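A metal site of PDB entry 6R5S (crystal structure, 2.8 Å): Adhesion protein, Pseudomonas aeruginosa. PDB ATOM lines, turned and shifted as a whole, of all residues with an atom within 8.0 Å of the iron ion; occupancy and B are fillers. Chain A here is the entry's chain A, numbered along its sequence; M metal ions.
A ring nitrogen (ND1) of His 111 is in hydrogen-bond range of the backbone carbonyl oxygen (O) of Gly 178, 3.1 Å away.
ND1 of His 111 is in hydrogen-bond range of ND2 of Asn 109, 2.7 Å away.
ND1 of His 41 lies within hydrogen-bond range of OD1 of Asn 39, at 2.7 Å.
A ring nitrogen (ND1) of His 177 is in hydrogen-bond range of the side-chain carboxylate (OE1) of Glu 196 (3.1 Å).
Of the 21 residues printed, 6 come within 4 Å of the iron ion.
The nearest printed residue that does not touch the iron ion is Ala 179 (5.1 Å).
NE2 of His 199 is bound to the iron ion, 2.2 Å away.
The iron ion is bound by NE2 of His 111, at 2.2 Å.
The iron ion is bound by NE2 of His 250.
NE2 of His 41 is bound to the iron ion (2.3 Å).
The iron ion is bound by NE2 of His 66.
The iron ion is bound by a ring nitrogen (NE2) of His 177, 2.4 Å away.
The iron ion has six donor atoms within binding distance.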
ATOM      1  N   LEU A  13     -11.348   6.171 -29.281  1.00  0.00           N
ATOM      2  CA  LEU A  13     -12.551   5.367 -29.057  1.00  0.00           C
ATOM      3  C   LEU A  13     -13.521   6.067 -28.107  1.00  0.00           C
ATOM      4  O   LEU A  13     -13.136   7.002 -27.407  1.00  0.00           O
ATOM      5  CB  LEU A  13     -12.185   3.942 -28.556  1.00  0.00           C
ATOM      6  CG  LEU A  13     -11.084   3.185 -29.341  1.00  0.00           C
ATOM      7  CD1 LEU A  13     -10.648   1.936 -28.602  1.00  0.00           C
ATOM      8  CD2 LEU A  13     -11.523   2.838 -30.757  1.00  0.00           C
ATOM      9  N   ASN A  39     -17.584   2.804 -37.379  1.00  0.00           N
ATOM     10  CA  ASN A  39     -17.187   1.605 -36.664  1.00  0.00           C
ATOM     11  C   ASN A  39     -15.671   1.711 -36.568  1.00  0.00           C
ATOM     12  O   ASN A  39     -15.016   1.830 -37.602  1.00  0.00           O
ATOM     13  CB  ASN A  39     -17.581   0.357 -37.455  1.00  0.00           C
ATOM     14  CG  ASN A  39     -17.454  -0.931 -36.687  1.00  0.00           C
ATOM     15  OD1 ASN A  39     -16.646  -1.087 -35.776  1.00  0.00           O
ATOM     16  ND2 ASN A  39     -18.256  -1.899 -37.051  1.00  0.00           N
ATOM     17  N   PRO A  40     -15.073   1.716 -35.338  1.00  0.00           N
ATOM     18  CA  PRO A  40     -13.601   1.860 -35.242  1.00  0.00           C
ATOM     19  C   PRO A  40     -12.792   0.709 -35.862  1.00  0.00           C
ATOM     20  O   PRO A  40     -11.643   0.938 -36.267  1.00  0.00           O
ATOM     21  CB  PRO A  40     -13.357   2.009 -33.744  1.00  0.00           C
ATOM     22  CG  PRO A  40     -14.559   1.407 -33.091  1.00  0.00           C
ATOM     23  CD  PRO A  40     -15.712   1.623 -34.014  1.00  0.00           C
ATOM     24  N   HIS A  41     -13.389  -0.506 -35.993  1.00  0.00           N
ATOM     25  CA  HIS A  41     -12.777  -1.678 -36.631  1.00  0.00           C
ATOM     26  C   HIS A  41     -12.705  -1.478 -38.149  1.00  0.00           C
ATOM     27  O   HIS A  41     -11.709  -1.852 -38.772  1.00  0.00           O
ATOM     28  CB  HIS A  41     -13.614  -2.937 -36.325  1.00  0.00           C
ATOM     29  CG  HIS A  41     -13.877  -3.165 -34.865  1.00  0.00           C
ATOM     30  ND1 HIS A  41     -14.931  -2.547 -34.217  1.00  0.00           N
ATOM     31  CD2 HIS A  41     -13.212  -3.915 -33.972  1.00  0.00           C
ATOM     32  CE1 HIS A  41     -14.883  -2.957 -32.974  1.00  0.00           C
ATOM     33  NE2 HIS A  41     -13.860  -3.777 -32.771  1.00  0.00           N
ATOM     34  N   GLY A  65      -3.707  -2.292 -29.333  1.00  0.00           N
ATOM     35  CA  GLY A  65      -4.304  -2.908 -30.507  1.00  0.00           C
ATOM     36  C   GLY A  65      -5.702  -2.483 -30.911  1.00  0.00           C
ATOM     37  O   GLY A  65      -6.272  -3.073 -31.825  1.00  0.00           O
ATOM     38  N   HIS A  66      -6.257  -1.458 -30.252  1.00  0.00           N
ATOM     39  CA  HIS A  66      -7.596  -1.012 -30.624  1.00  0.00           C
ATOM     40  C   HIS A  66      -7.619   0.391 -31.255  1.00  0.00           C
ATOM     41  O   HIS A  66      -8.694   0.948 -31.471  1.00  0.00           O
ATOM     42  CB  HIS A  66      -8.601  -1.139 -29.476  1.00  0.00           C
ATOM     43  CG  HIS A  66      -9.924  -1.653 -29.950  1.00  0.00           C
ATOM     44  ND1 HIS A  66     -10.613  -1.053 -30.987  1.00  0.00           N
ATOM     45  CD2 HIS A  66     -10.647  -2.700 -29.491  1.00  0.00           C
ATOM     46  CE1 HIS A  66     -11.721  -1.749 -31.130  1.00  0.00           C
ATOM     47  NE2 HIS A  66     -11.780  -2.756 -30.260  1.00  0.00           N
ATOM     48  N   ASN A 109      -5.376  -8.980 -26.043  1.00  0.00           N
ATOM     49  CA  ASN A 109      -6.759  -8.536 -26.121  1.00  0.00           C
ATOM     50  C   ASN A 109      -6.765  -6.989 -25.793  1.00  0.00           C
ATOM     51  O   ASN A 109      -6.360  -6.579 -24.684  1.00  0.00           O
ATOM     52  CB  ASN A 109      -7.655  -9.374 -25.189  1.00  0.00           C
ATOM     53  CG  ASN A 109      -9.152  -9.145 -25.327  1.00  0.00           C
ATOM     54  OD1 ASN A 109      -9.975 -10.021 -25.000  1.00  0.00           O
ATOM     55  ND2 ASN A 109      -9.571  -7.982 -25.782  1.00  0.00           N
ATOM     56  N   PRO A 110      -7.138  -6.113 -26.765  1.00  0.00           N
ATOM     57  CA  PRO A 110      -7.081  -4.670 -26.521  1.00  0.00           C
ATOM     58  C   PRO A 110      -8.278  -4.057 -25.812  1.00  0.00           C
ATOM     59  O   PRO A 110      -8.287  -2.852 -25.596  1.00  0.00           O
ATOM     60  CB  PRO A 110      -6.942  -4.103 -27.941  1.00  0.00           C
ATOM     61  CG  PRO A 110      -7.689  -5.066 -28.805  1.00  0.00           C
ATOM     62  CD  PRO A 110      -7.580  -6.407 -28.155  1.00  0.00           C
ATOM     63  N   HIS A 111      -9.288  -4.874 -25.445  1.00  0.00           N
ATOM     64  CA  HIS A 111     -10.536  -4.417 -24.833  1.00  0.00           C
ATOM     65  C   HIS A 111     -10.500  -4.257 -23.321  1.00  0.00           C
ATOM     66  O   HIS A 111     -11.427  -4.674 -22.626  1.00  0.00           O
ATOM     67  CB  HIS A 111     -11.698  -5.333 -25.249  1.00  0.00           C
ATOM     68  CG  HIS A 111     -11.839  -5.517 -26.731  1.00  0.00           C
ATOM     69  ND1 HIS A 111     -11.188  -6.537 -27.382  1.00  0.00           N
ATOM     70  CD2 HIS A 111     -12.588  -4.829 -27.618  1.00  0.00           C
ATOM     71  CE1 HIS A 111     -11.563  -6.455 -28.653  1.00  0.00           C
ATOM     72  NE2 HIS A 111     -12.404  -5.449 -28.835  1.00  0.00           N
ATOM     73  N   PHE A 113     -10.786  -1.359 -21.724  1.00  0.00           N
ATOM     74  CA  PHE A 113     -11.894  -0.448 -21.452  1.00  0.00           C
ATOM     75  C   PHE A 113     -13.244  -1.133 -21.133  1.00  0.00           C
ATOM     76  O   PHE A 113     -14.125  -0.464 -20.572  1.00  0.00           O
ATOM     77  CB  PHE A 113     -12.086   0.582 -22.580  1.00  0.00           C
ATOM     78  CG  PHE A 113     -12.145  -0.001 -23.973  1.00  0.00           C
ATOM     79  CD1 PHE A 113     -13.353  -0.407 -24.512  1.00  0.00           C
ATOM     80  CD2 PHE A 113     -11.008  -0.068 -24.766  1.00  0.00           C
ATOM     81  CE1 PHE A 113     -13.412  -0.944 -25.794  1.00  0.00           C
ATOM     82  CE2 PHE A 113     -11.069  -0.586 -26.056  1.00  0.00           C
ATOM     83  CZ  PHE A 113     -12.280  -1.022 -26.563  1.00  0.00           C
ATOM     84  N   LEU A 114     -13.438  -2.428 -21.449  1.00  0.00           N
ATOM     85  CA  LEU A 114     -14.698  -3.078 -21.075  1.00  0.00           C
ATOM     86  C   LEU A 114     -14.528  -3.856 -19.757  1.00  0.00           C
ATOM     87  O   LEU A 114     -15.055  -4.953 -19.605  1.00  0.00           O
ATOM     88  CB  LEU A 114     -15.339  -3.910 -22.204  1.00  0.00           C
ATOM     89  CG  LEU A 114     -15.524  -3.191 -23.554  1.00  0.00           C
ATOM     90  CD1 LEU A 114     -15.803  -4.152 -24.660  1.00  0.00           C
ATOM     91  CD2 LEU A 114     -16.586  -2.080 -23.495  1.00  0.00           C
ATOM     92  N   HIS A 177     -17.710 -11.393 -30.651  1.00  0.00           N
ATOM     93  CA  HIS A 177     -16.547 -10.518 -30.616  1.00  0.00           C
ATOM     94  C   HIS A 177     -15.673 -10.858 -29.386  1.00  0.00           C
ATOM     95  O   HIS A 177     -16.203 -11.119 -28.311  1.00  0.00           O
ATOM     96  CB  HIS A 177     -17.051  -9.047 -30.524  1.00  0.00           C
ATOM     97  CG  HIS A 177     -16.060  -8.025 -30.997  1.00  0.00           C
ATOM     98  ND1 HIS A 177     -15.854  -7.796 -32.333  1.00  0.00           N
ATOM     99  CD2 HIS A 177     -15.290  -7.184 -30.276  1.00  0.00           C
ATOM    100  CE1 HIS A 177     -14.923  -6.847 -32.390  1.00  0.00           C
ATOM    101  NE2 HIS A 177     -14.569  -6.433 -31.179  1.00  0.00           N
ATOM    102  N   GLY A 178     -14.359 -10.814 -29.528  1.00  0.00           N
ATOM    103  CA  GLY A 178     -13.434 -11.092 -28.424  1.00  0.00           C
ATOM    104  C   GLY A 178     -13.196  -9.881 -27.543  1.00  0.00           C
ATOM    105  O   GLY A 178     -12.053  -9.512 -27.277  1.00  0.00           O
ATOM    106  N   ALA A 179     -14.292  -9.284 -27.060  1.00  0.00           N
ATOM    107  CA  ALA A 179     -14.264  -8.064 -26.248  1.00  0.00           C
ATOM    108  C   ALA A 179     -14.630  -8.198 -24.766  1.00  0.00           C
ATOM    109  O   ALA A 179     -14.494  -7.189 -24.049  1.00  0.00           O
ATOM    110  CB  ALA A 179     -15.202  -7.046 -26.889  1.00  0.00           C
ATOM    111  N   TYR A 180     -15.120  -9.358 -24.282  1.00  0.00           N
ATOM    112  CA  TYR A 180     -15.665  -9.419 -22.936  1.00  0.00           C
ATOM    113  C   TYR A 180     -14.866 -10.228 -21.912  1.00  0.00           C
ATOM    114  O   TYR A 180     -15.300 -10.345 -20.761  1.00  0.00           O
ATOM    115  CB  TYR A 180     -17.125  -9.877 -23.031  1.00  0.00           C
ATOM    116  CG  TYR A 180     -17.886  -8.980 -23.987  1.00  0.00           C
ATOM    117  CD1 TYR A 180     -18.163  -7.651 -23.653  1.00  0.00           C
ATOM    118  CD2 TYR A 180     -18.170  -9.401 -25.290  1.00  0.00           C
ATOM    119  CE1 TYR A 180     -18.742  -6.789 -24.567  1.00  0.00           C
ATOM    120  CE2 TYR A 180     -18.759  -8.533 -26.211  1.00  0.00           C
ATOM    121  CZ  TYR A 180     -19.053  -7.234 -25.839  1.00  0.00           C
ATOM    122  OH  TYR A 180     -19.669  -6.371 -26.714  1.00  0.00           O
ATOM    123  N   GLU A 196     -15.525 -15.048 -33.618  1.00  0.00           N
ATOM    124  CA  GLU A 196     -14.652 -14.384 -34.591  1.00  0.00           C
ATOM    125  C   GLU A 196     -13.219 -14.972 -34.508  1.00  0.00           C
ATOM    126  O   GLU A 196     -12.607 -14.923 -33.438  1.00  0.00           O
ATOM    127  CB  GLU A 196     -14.685 -12.858 -34.409  1.00  0.00           C
ATOM    128  CG  GLU A 196     -16.024 -12.227 -34.835  1.00  0.00           C
ATOM    129  CD  GLU A 196     -16.157 -10.712 -34.907  1.00  0.00           C
ATOM    130  OE1 GLU A 196     -15.252  -9.979 -34.432  1.00  0.00           O
ATOM    131  OE2 GLU A 196     -17.178 -10.247 -35.460  1.00  0.00           O
ATOM    132  N   HIS A 199      -9.649 -10.611 -34.101  1.00  0.00           N
ATOM    133  CA  HIS A 199     -10.381  -9.387 -33.772  1.00  0.00           C
ATOM    134  C   HIS A 199     -11.006  -8.736 -35.018  1.00  0.00           C
ATOM    135  O   HIS A 199     -10.312  -8.556 -35.997  1.00  0.00           O
ATOM    136  CB  HIS A 199      -9.451  -8.423 -33.041  1.00  0.00           C
ATOM    137  CG  HIS A 199     -10.087  -7.179 -32.511  1.00  0.00           C
ATOM    138  ND1 HIS A 199      -9.368  -5.996 -32.416  1.00  0.00           N
ATOM    139  CD2 HIS A 199     -11.332  -6.968 -32.043  1.00  0.00           C
ATOM    140  CE1 HIS A 199     -10.191  -5.112 -31.880  1.00  0.00           C
ATOM    141  NE2 HIS A 199     -11.382  -5.643 -31.633  1.00  0.00           N
ATOM    142  N   GLY A 200     -12.314  -8.466 -34.986  1.00  0.00           N
ATOM    143  CA  GLY A 200     -13.065  -7.827 -36.066  1.00  0.00           C
ATOM    144  C   GLY A 200     -13.110  -8.587 -37.389  1.00  0.00           C
ATOM    145  O   GLY A 200     -13.461  -8.002 -38.433  1.00  0.00           O
ATOM    146  N   GLU A 226     -23.360  -8.884 -30.326  1.00  0.00           N
ATOM    147  CA  GLU A 226     -23.141  -7.444 -30.424  1.00  0.00           C
ATOM    148  C   GLU A 226     -24.415  -6.583 -30.610  1.00  0.00           C
ATOM    149  O   GLU A 226     -25.174  -6.785 -31.555  1.00  0.00           O
ATOM    150  CB  GLU A 226     -22.143  -7.132 -31.548  1.00  0.00           C
ATOM    151  CG  GLU A 226     -20.693  -7.191 -31.121  1.00  0.00           C
ATOM    152  CD  GLU A 226     -20.230  -6.282 -29.989  1.00  0.00           C
ATOM    153  OE1 GLU A 226     -20.721  -5.141 -29.854  1.00  0.00           O
ATOM    154  OE2 GLU A 226     -19.342  -6.745 -29.233  1.00  0.00           O
ATOM    155  N   HIS A 250     -20.015  -2.885 -27.024  1.00  0.00           N
ATOM    156  CA  HIS A 250     -18.589  -2.610 -27.172  1.00  0.00           C
ATOM    157  C   HIS A 250     -18.340  -1.128 -26.791  1.00  0.00           C
ATOM    158  O   HIS A 250     -17.191  -0.755 -26.571  1.00  0.00           O
ATOM    159  CB  HIS A 250     -18.211  -2.875 -28.644  1.00  0.00           C
ATOM    160  CG  HIS A 250     -16.745  -2.998 -28.945  1.00  0.00           C
ATOM    161  ND1 HIS A 250     -15.871  -1.956 -28.712  1.00  0.00           N
ATOM    162  CD2 HIS A 250     -16.081  -3.992 -29.563  1.00  0.00           C
ATOM    163  CE1 HIS A 250     -14.697  -2.358 -29.170  1.00  0.00           C
ATOM    164  NE2 HIS A 250     -14.780  -3.573 -29.695  1.00  0.00           N
ATOM    165  N   SER A 252     -19.211   1.769 -28.752  1.00  0.00           N
ATOM    166  CA  SER A 252     -18.620   2.271 -30.000  1.00  0.00           C
ATOM    167  C   SER A 252     -19.624   2.861 -30.987  1.00  0.00           C
ATOM    168  O   SER A 252     -19.217   3.392 -32.031  1.00  0.00           O
ATOM    169  CB  SER A 252     -17.819   1.157 -30.685  1.00  0.00           C
ATOM    170  OG  SER A 252     -18.636   0.110 -31.180  1.00  0.00           O
HETATM  171 FE    FE M   1     -13.077  -4.607 -30.779  1.00  0.00          FE
